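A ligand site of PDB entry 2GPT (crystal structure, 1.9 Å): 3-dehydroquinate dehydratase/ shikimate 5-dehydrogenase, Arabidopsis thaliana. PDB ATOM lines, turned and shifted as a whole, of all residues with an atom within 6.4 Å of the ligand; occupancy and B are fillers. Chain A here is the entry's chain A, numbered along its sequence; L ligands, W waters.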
ATOM      1  N   ILE A 239       9.695 -14.397 -22.053  1.00  0.00           N
ATOM      2  CA  ILE A 239       8.996 -13.759 -23.159  1.00  0.00           C
ATOM      3  C   ILE A 239       9.973 -12.798 -23.840  1.00  0.00           C
ATOM      4  O   ILE A 239      10.526 -11.890 -23.212  1.00  0.00           O
ATOM      5  CB  ILE A 239       7.739 -12.980 -22.680  1.00  0.00           C
ATOM      6  CG1 ILE A 239       7.230 -12.086 -23.805  1.00  0.00           C
ATOM      7  CG2 ILE A 239       8.063 -12.176 -21.438  1.00  0.00           C
ATOM      8  CD1 ILE A 239       6.784 -12.828 -25.070  1.00  0.00           C
ATOM      9  N   VAL A 244       8.637  -5.166 -23.423  1.00  0.00           N
ATOM     10  CA  VAL A 244       8.263  -6.427 -22.793  1.00  0.00           C
ATOM     11  C   VAL A 244       7.750  -6.252 -21.365  1.00  0.00           C
ATOM     12  O   VAL A 244       7.194  -7.175 -20.789  1.00  0.00           O
ATOM     13  CB  VAL A 244       9.493  -7.386 -22.768  1.00  0.00           C
ATOM     14  CG1 VAL A 244      10.498  -6.896 -21.750  1.00  0.00           C
ATOM     15  CG2 VAL A 244       9.048  -8.797 -22.447  1.00  0.00           C
ATOM     16  N   HIS A 246       5.216  -4.927 -20.142  1.00  0.00           N
ATOM     17  CA  HIS A 246       3.774  -5.100 -19.964  1.00  0.00           C
ATOM     18  C   HIS A 246       3.345  -6.564 -19.877  1.00  0.00           C
ATOM     19  O   HIS A 246       2.266  -6.871 -19.382  1.00  0.00           O
ATOM     20  CB  HIS A 246       3.042  -4.499 -21.148  1.00  0.00           C
ATOM     21  CG  HIS A 246       3.363  -5.204 -22.424  1.00  0.00           C
ATOM     22  ND1 HIS A 246       4.559  -5.028 -23.084  1.00  0.00           N
ATOM     23  CD2 HIS A 246       2.700  -6.177 -23.095  1.00  0.00           C
ATOM     24  CE1 HIS A 246       4.620  -5.880 -24.103  1.00  0.00           C
ATOM     25  NE2 HIS A 246       3.504  -6.579 -24.127  1.00  0.00           N
ATOM     26  N   SER A 247       4.174  -7.464 -20.399  1.00  0.00           N
ATOM     27  CA  SER A 247       3.818  -8.883 -20.440  1.00  0.00           C
ATOM     28  C   SER A 247       3.436  -9.568 -19.141  1.00  0.00           C
ATOM     29  O   SER A 247       4.086  -9.389 -18.114  1.00  0.00           O
ATOM     30  CB  SER A 247       4.920  -9.691 -21.101  1.00  0.00           C
ATOM     31  OG  SER A 247       4.583 -11.068 -21.064  1.00  0.00           O
ATOM     32  N   LYS A 248       2.390 -10.379 -19.196  1.00  0.00           N
ATOM     33  CA  LYS A 248       1.948 -11.109 -18.029  1.00  0.00           C
ATOM     34  C   LYS A 248       2.260 -12.592 -18.201  1.00  0.00           C
ATOM     35  O   LYS A 248       1.783 -13.429 -17.416  1.00  0.00           O
ATOM     36  CB  LYS A 248       0.450 -10.905 -17.787  1.00  0.00           C
ATOM     37  CG  LYS A 248       0.098  -9.493 -17.355  1.00  0.00           C
ATOM     38  CD  LYS A 248      -1.395  -9.344 -17.000  1.00  0.00           C
ATOM     39  CE  LYS A 248      -1.690  -7.952 -16.463  1.00  0.00           C
ATOM     40  NZ  LYS A 248      -3.144  -7.696 -16.221  1.00  0.00           N
ATOM     41  N   SER A 249       3.038 -12.946 -19.229  1.00  0.00           N
ATOM     42  CA  SER A 249       3.415 -14.338 -19.442  1.00  0.00           C
ATOM     43  C   SER A 249       4.197 -14.833 -18.211  1.00  0.00           C
ATOM     44  O   SER A 249       4.081 -15.994 -17.811  1.00  0.00           O
ATOM     45  CB  SER A 249       4.248 -14.505 -20.711  1.00  0.00           C
ATOM     46  OG  SER A 249       3.421 -14.522 -21.866  1.00  0.00           O
ATOM     47  N   PRO A 250       5.036 -13.964 -17.629  1.00  0.00           N
ATOM     48  CA  PRO A 250       5.783 -14.410 -16.447  1.00  0.00           C
ATOM     49  C   PRO A 250       4.848 -14.748 -15.270  1.00  0.00           C
ATOM     50  O   PRO A 250       5.145 -15.612 -14.454  1.00  0.00           O
ATOM     51  CB  PRO A 250       6.693 -13.213 -16.146  1.00  0.00           C
ATOM     52  CG  PRO A 250       7.050 -12.743 -17.506  1.00  0.00           C
ATOM     53  CD  PRO A 250       5.694 -12.796 -18.244  1.00  0.00           C
ATOM     54  N   TYR A 266      10.153 -18.563 -15.443  1.00  0.00           N
ATOM     55  CA  TYR A 266       9.852 -17.735 -16.603  1.00  0.00           C
ATOM     56  C   TYR A 266      10.116 -16.248 -16.298  1.00  0.00           C
ATOM     57  O   TYR A 266       9.645 -15.726 -15.288  1.00  0.00           O
ATOM     58  CB  TYR A 266       8.392 -17.954 -16.992  1.00  0.00           C
ATOM     59  CG  TYR A 266       8.011 -17.503 -18.384  1.00  0.00           C
ATOM     60  CD1 TYR A 266       7.842 -16.151 -18.683  1.00  0.00           C
ATOM     61  CD2 TYR A 266       7.790 -18.436 -19.413  1.00  0.00           C
ATOM     62  CE1 TYR A 266       7.453 -15.733 -19.947  1.00  0.00           C
ATOM     63  CE2 TYR A 266       7.406 -18.025 -20.681  1.00  0.00           C
ATOM     64  CZ  TYR A 266       7.238 -16.672 -20.940  1.00  0.00           C
ATOM     65  OH  TYR A 266       6.836 -16.251 -22.178  1.00  0.00           O
ATOM     66  N   SER A 290       8.910 -17.484 -25.548  1.00  0.00           N
ATOM     67  CA  SER A 290       7.662 -17.020 -26.144  1.00  0.00           C
ATOM     68  C   SER A 290       8.140 -15.792 -26.917  1.00  0.00           C
ATOM     69  O   SER A 290       9.111 -15.152 -26.520  1.00  0.00           O
ATOM     70  CB  SER A 290       6.641 -16.593 -25.084  1.00  0.00           C
ATOM     71  OG  SER A 290       6.267 -17.680 -24.249  1.00  0.00           O
ATOM     72  N   CYS A 291       7.482 -15.476 -28.021  1.00  0.00           N
ATOM     73  CA  CYS A 291       7.899 -14.322 -28.817  1.00  0.00           C
ATOM     74  C   CYS A 291       6.760 -13.390 -29.152  1.00  0.00           C
ATOM     75  O   CYS A 291       5.703 -13.837 -29.600  1.00  0.00           O
ATOM     76  CB  CYS A 291       8.556 -14.784 -30.121  1.00  0.00           C
ATOM     77  SG  CYS A 291       9.963 -15.872 -29.916  1.00  0.00           S
ATOM     78  N   THR A 292       6.973 -12.105 -28.931  1.00  0.00           N
ATOM     79  CA  THR A 292       5.964 -11.113 -29.261  1.00  0.00           C
ATOM     80  C   THR A 292       6.637 -10.035 -30.115  1.00  0.00           C
ATOM     81  O   THR A 292       7.789 -10.195 -30.519  1.00  0.00           O
ATOM     82  CB  THR A 292       5.350 -10.497 -27.992  1.00  0.00           C
ATOM     83  OG1 THR A 292       4.235  -9.677 -28.359  1.00  0.00           O
ATOM     84  CG2 THR A 292       6.377  -9.629 -27.255  1.00  0.00           C
ATOM     85  N   ILE A 293       5.924  -8.951 -30.396  1.00  0.00           N
ATOM     86  CA  ILE A 293       6.484  -7.877 -31.204  1.00  0.00           C
ATOM     87  C   ILE A 293       7.843  -7.485 -30.640  1.00  0.00           C
ATOM     88  O   ILE A 293       8.005  -7.347 -29.438  1.00  0.00           O
ATOM     89  CB  ILE A 293       5.544  -6.642 -31.205  1.00  0.00           C
ATOM     90  CG1 ILE A 293       4.168  -7.044 -31.730  1.00  0.00           C
ATOM     91  CG2 ILE A 293       6.126  -5.527 -32.079  1.00  0.00           C
ATOM     92  CD1 ILE A 293       3.169  -5.923 -31.732  1.00  0.00           C
ATOM     93  N   LYS A 296       8.247 -12.068 -33.701  1.00  0.00           N
ATOM     94  CA  LYS A 296       7.481 -13.235 -34.122  1.00  0.00           C
ATOM     95  C   LYS A 296       7.940 -13.731 -35.495  1.00  0.00           C
ATOM     96  O   LYS A 296       8.250 -14.907 -35.671  1.00  0.00           O
ATOM     97  CB  LYS A 296       5.987 -12.910 -34.189  1.00  0.00           C
ATOM     98  CG  LYS A 296       5.336 -12.633 -32.861  1.00  0.00           C
ATOM     99  CD  LYS A 296       3.865 -12.274 -33.065  1.00  0.00           C
ATOM    100  CE  LYS A 296       3.147 -12.107 -31.751  1.00  0.00           C
ATOM    101  NZ  LYS A 296       3.188 -13.372 -30.959  1.00  0.00           N
ATOM    102  N   ASN A 317       5.765 -17.844 -32.594  1.00  0.00           N
ATOM    103  CA  ASN A 317       5.565 -17.141 -31.326  1.00  0.00           C
ATOM    104  C   ASN A 317       5.974 -18.026 -30.143  1.00  0.00           C
ATOM    105  O   ASN A 317       5.822 -17.637 -28.983  1.00  0.00           O
ATOM    106  CB  ASN A 317       4.107 -16.691 -31.140  1.00  0.00           C
ATOM    107  CG  ASN A 317       3.221 -17.763 -30.536  1.00  0.00           C
ATOM    108  OD1 ASN A 317       2.260 -17.456 -29.831  1.00  0.00           O
ATOM    109  ND2 ASN A 317       3.526 -19.020 -30.818  1.00  0.00           N
ATOM    110  N   THR A 318       6.482 -19.224 -30.454  1.00  0.00           N
ATOM    111  CA  THR A 318       6.920 -20.157 -29.419  1.00  0.00           C
ATOM    112  C   THR A 318       8.151 -20.931 -29.848  1.00  0.00           C
ATOM    113  O   THR A 318       8.148 -21.613 -30.879  1.00  0.00           O
ATOM    114  CB  THR A 318       5.813 -21.202 -29.102  1.00  0.00           C
ATOM    115  OG1 THR A 318       4.535 -20.568 -29.059  1.00  0.00           O
ATOM    116  CG2 THR A 318       6.094 -21.865 -27.763  1.00  0.00           C
ATOM    117  N   THR A 333       1.171 -20.588 -31.546  1.00  0.00           N
ATOM    118  CA  THR A 333      -0.029 -20.788 -30.749  1.00  0.00           C
ATOM    119  C   THR A 333      -0.966 -19.593 -30.872  1.00  0.00           C
ATOM    120  O   THR A 333      -2.030 -19.563 -30.246  1.00  0.00           O
ATOM    121  CB  THR A 333       0.320 -20.999 -29.265  1.00  0.00           C
ATOM    122  OG1 THR A 333       0.899 -19.799 -28.737  1.00  0.00           O
ATOM    123  CG2 THR A 333       1.323 -22.147 -29.113  1.00  0.00           C
ATOM    124  N   ASP A 334      -0.575 -18.603 -31.663  1.00  0.00           N
ATOM    125  CA  ASP A 334      -1.409 -17.412 -31.852  1.00  0.00           C
ATOM    126  C   ASP A 334      -2.652 -17.733 -32.669  1.00  0.00           C
ATOM    127  O   ASP A 334      -3.756 -17.286 -32.336  1.00  0.00           O
ATOM    128  CB  ASP A 334      -0.620 -16.306 -32.559  1.00  0.00           C
ATOM    129  CG  ASP A 334       0.282 -15.527 -31.613  1.00  0.00           C
ATOM    130  OD1 ASP A 334      -0.205 -15.071 -30.556  1.00  0.00           O
ATOM    131  OD2 ASP A 334       1.486 -15.366 -31.930  1.00  0.00           O
ATOM    132  N   ALA A 375       1.195 -11.569 -35.503  1.00  0.00           N
ATOM    133  CA  ALA A 375      -0.144 -11.826 -34.973  1.00  0.00           C
ATOM    134  C   ALA A 375      -1.178 -11.697 -36.093  1.00  0.00           C
ATOM    135  O   ALA A 375      -2.153 -12.443 -36.143  1.00  0.00           O
ATOM    136  CB  ALA A 375      -0.451 -10.857 -33.848  1.00  0.00           C
ATOM    137  N   TYR A 461      -3.927  -7.061 -24.540  1.00  0.00           N
ATOM    138  CA  TYR A 461      -4.569  -7.434 -23.285  1.00  0.00           C
ATOM    139  C   TYR A 461      -4.150  -6.535 -22.124  1.00  0.00           C
ATOM    140  O   TYR A 461      -4.614  -6.712 -20.991  1.00  0.00           O
ATOM    141  CB  TYR A 461      -4.318  -8.915 -22.936  1.00  0.00           C
ATOM    142  CG  TYR A 461      -2.881  -9.287 -22.660  1.00  0.00           C
ATOM    143  CD1 TYR A 461      -1.961  -9.452 -23.707  1.00  0.00           C
ATOM    144  CD2 TYR A 461      -2.430  -9.472 -21.350  1.00  0.00           C
ATOM    145  CE1 TYR A 461      -0.633  -9.773 -23.447  1.00  0.00           C
ATOM    146  CE2 TYR A 461      -1.104  -9.799 -21.082  1.00  0.00           C
ATOM    147  CZ  TYR A 461      -0.213  -9.940 -22.131  1.00  0.00           C
ATOM    148  OH  TYR A 461       1.093 -10.261 -21.850  1.00  0.00           O
ATOM    149  N   MET A 485      -7.627 -14.582 -25.920  1.00  0.00           N
ATOM    150  CA  MET A 485      -6.626 -15.135 -26.824  1.00  0.00           C
ATOM    151  C   MET A 485      -5.326 -15.403 -26.071  1.00  0.00           C
ATOM    152  O   MET A 485      -4.624 -16.383 -26.337  1.00  0.00           O
ATOM    153  CB  MET A 485      -6.375 -14.157 -27.976  1.00  0.00           C
ATOM    154  CG  MET A 485      -5.149 -14.489 -28.852  1.00  0.00           C
ATOM    155  SD  MET A 485      -3.525 -14.159 -28.069  1.00  0.00           S
ATOM    156  CE  MET A 485      -3.452 -12.347 -28.117  1.00  0.00           C
ATOM    157  N   PHE A 486      -5.012 -14.517 -25.132  1.00  0.00           N
ATOM    158  CA  PHE A 486      -3.780 -14.667 -24.355  1.00  0.00           C
ATOM    159  C   PHE A 486      -3.745 -15.951 -23.540  1.00  0.00           C
ATOM    160  O   PHE A 486      -2.761 -16.695 -23.580  1.00  0.00           O
ATOM    161  CB  PHE A 486      -3.601 -13.487 -23.401  1.00  0.00           C
ATOM    162  CG  PHE A 486      -2.335 -13.573 -22.589  1.00  0.00           C
ATOM    163  CD1 PHE A 486      -1.097 -13.375 -23.182  1.00  0.00           C
ATOM    164  CD2 PHE A 486      -2.389 -13.851 -21.229  1.00  0.00           C
ATOM    165  CE1 PHE A 486       0.088 -13.450 -22.423  1.00  0.00           C
ATOM    166  CE2 PHE A 486      -1.225 -13.942 -20.463  1.00  0.00           C
ATOM    167  CZ  PHE A 486       0.015 -13.739 -21.063  1.00  0.00           C
ATOM    168  N   GLN A 489      -3.540 -19.157 -25.972  1.00  0.00           N
ATOM    169  CA  GLN A 489      -2.224 -19.384 -26.555  1.00  0.00           C
ATOM    170  C   GLN A 489      -1.202 -19.698 -25.469  1.00  0.00           C
ATOM    171  O   GLN A 489      -0.188 -20.364 -25.727  1.00  0.00           O
ATOM    172  CB  GLN A 489      -1.788 -18.177 -27.395  1.00  0.00           C
ATOM    173  CG  GLN A 489      -1.525 -16.874 -26.635  1.00  0.00           C
ATOM    174  CD  GLN A 489      -0.207 -16.900 -25.892  1.00  0.00           C
ATOM    175  OE1 GLN A 489       0.802 -17.398 -26.397  1.00  0.00           O
ATOM    176  NE2 GLN A 489      -0.199 -16.341 -24.684  1.00  0.00           N
ATOM    177  N   GLN A 493       1.418 -23.108 -24.947  1.00  0.00           N
ATOM    178  CA  GLN A 493       2.859 -22.967 -24.849  1.00  0.00           C
ATOM    179  C   GLN A 493       3.372 -23.816 -23.687  1.00  0.00           C
ATOM    180  O   GLN A 493       4.435 -24.433 -23.748  1.00  0.00           O
ATOM    181  CB  GLN A 493       3.273 -21.513 -24.620  1.00  0.00           C
ATOM    182  CG  GLN A 493       2.885 -20.545 -25.705  1.00  0.00           C
ATOM    183  CD  GLN A 493       3.644 -19.228 -25.610  1.00  0.00           C
ATOM    184  OE1 GLN A 493       3.740 -18.623 -24.537  1.00  0.00           O
ATOM    185  NE2 GLN A 493       4.200 -18.776 -26.734  1.00  0.00           N
HETATM  186  O1  LIG L   1       1.909 -14.755 -28.799  1.00  0.00           O
HETATM  187  C1  LIG L   1       1.884 -14.233 -27.459  1.00  0.00           C
HETATM  188  C2  LIG L   1       3.276 -14.430 -26.793  1.00  0.00           C
HETATM  189  O2  LIG L   1       3.625 -15.821 -26.764  1.00  0.00           O
HETATM  190  C3  LIG L   1       3.262 -13.892 -25.345  1.00  0.00           C
HETATM  191  C4  LIG L   1       2.659 -12.503 -25.275  1.00  0.00           C
HETATM  192  C5  LIG L   1       2.954 -11.690 -24.073  1.00  0.00           C
HETATM  193  O3  LIG L   1       3.741 -12.187 -23.105  1.00  0.00           O
HETATM  194  O4  LIG L   1       2.492 -10.567 -23.954  1.00  0.00           O
HETATM  195  C6  LIG L   1       1.870 -11.995 -26.221  1.00  0.00           C
HETATM  196  C7  LIG L   1       1.492 -12.719 -27.493  1.00  0.00           C
HETATM  197  O5  LIG L   1       2.154 -12.075 -28.591  1.00  0.00           O
HETATM  198  O   HOH W   1       2.898  -8.669 -25.821  1.00  0.00           O
HETATM  199  O   HOH W   2      -0.397 -10.662 -29.828  1.00  0.00           O
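OG of Ser 247 sits at hydrogen-bond distance from O3 of the ligand (2.5 Å).
OH of Tyr 461 is in hydrogen-bond range of O4 of the ligand, at 2.5 Å.
OG of Ser 249 sits at hydrogen-bond distance from O3 of the ligand, 2.7 Å away.
OD1 of Asp 334 is in hydrogen-bond range of O1 of the ligand (2.8 Å).
The side-chain amino group of Lys 296 sits at hydrogen-bond distance from an oxygen (O1) of the ligand (2.9 Å).
An oxygen (O1) of the ligand lies within hydrogen-bond range of the side-chain amide oxygen (OD1) of Asn 317, 2.9 Å away.
An oxygen (O2) of the ligand lies within hydrogen-bond range of the side-chain amide nitrogen (NE2) of Gln 493, 3.0 Å away.
An oxygen (O5) of the ligand is in hydrogen-bond range of the side-chain hydroxyl (OG1) of Thr 292 (3.2 Å).
OE1 of Gln 489 is in hydrogen-bond range of O2 of the ligand, 3.3 Å away.
The side-chain carboxylate (OD2) of Asp 334 is in salt-bridge range of the side-chain amino group (NZ) of Lys 296.
The side-chain amide oxygen (OD1) of Asn 317 lies close to the side-chain carboxylate (OD2) of Asp 334, 3.1 Å away.
O of Asn 317 lies within hydrogen-bond range of N of Cys 291 (2.9 Å).
The side-chain amide nitrogen (ND2) of Asn 317 lies within hydrogen-bond range of the side-chain hydroxyl (OG1) of Thr 318, at 2.6 Å.
The side-chain amide oxygen of Gln 493 sits at hydrogen-bond distance from the side-chain hydroxyl of Ser 290 (2.7 Å).
NE2 of Gln 489 sits at hydrogen-bond distance from O of Phe 486 (2.8 Å).
The side-chain hydroxyl (OG1) of Thr 333 is in hydrogen-bond range of the backbone carbonyl oxygen (O) of Gln 489 (3.2 Å).
The side-chain hydroxyl (OH) of Tyr 266 lies close to the backbone NH (N) of Ile 239 (3.4 Å).
Water W1 lies within hydrogen-bond range of O4 of the ligand (2.7 Å), NE2 of His 246 (2.8 Å) and OG1 of Thr 292 (3.0 Å).
CG1 of Ile 239 touches O3 of the ligand, at 3.6 Å.
CB of Ser 290 touches O2 of the ligand, 3.5 Å away.
O of Cys 291 touches C2 of the ligand (3.8 Å).
CE1 of Phe 486 touches C5 of the ligand, 3.7 Å away.
Hydrophobic or aromatic side chains that line the ligand: Ile 239, Tyr 461 and Phe 486.
Of the 23 residues printed, 13 come within 4 Å of the ligand.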
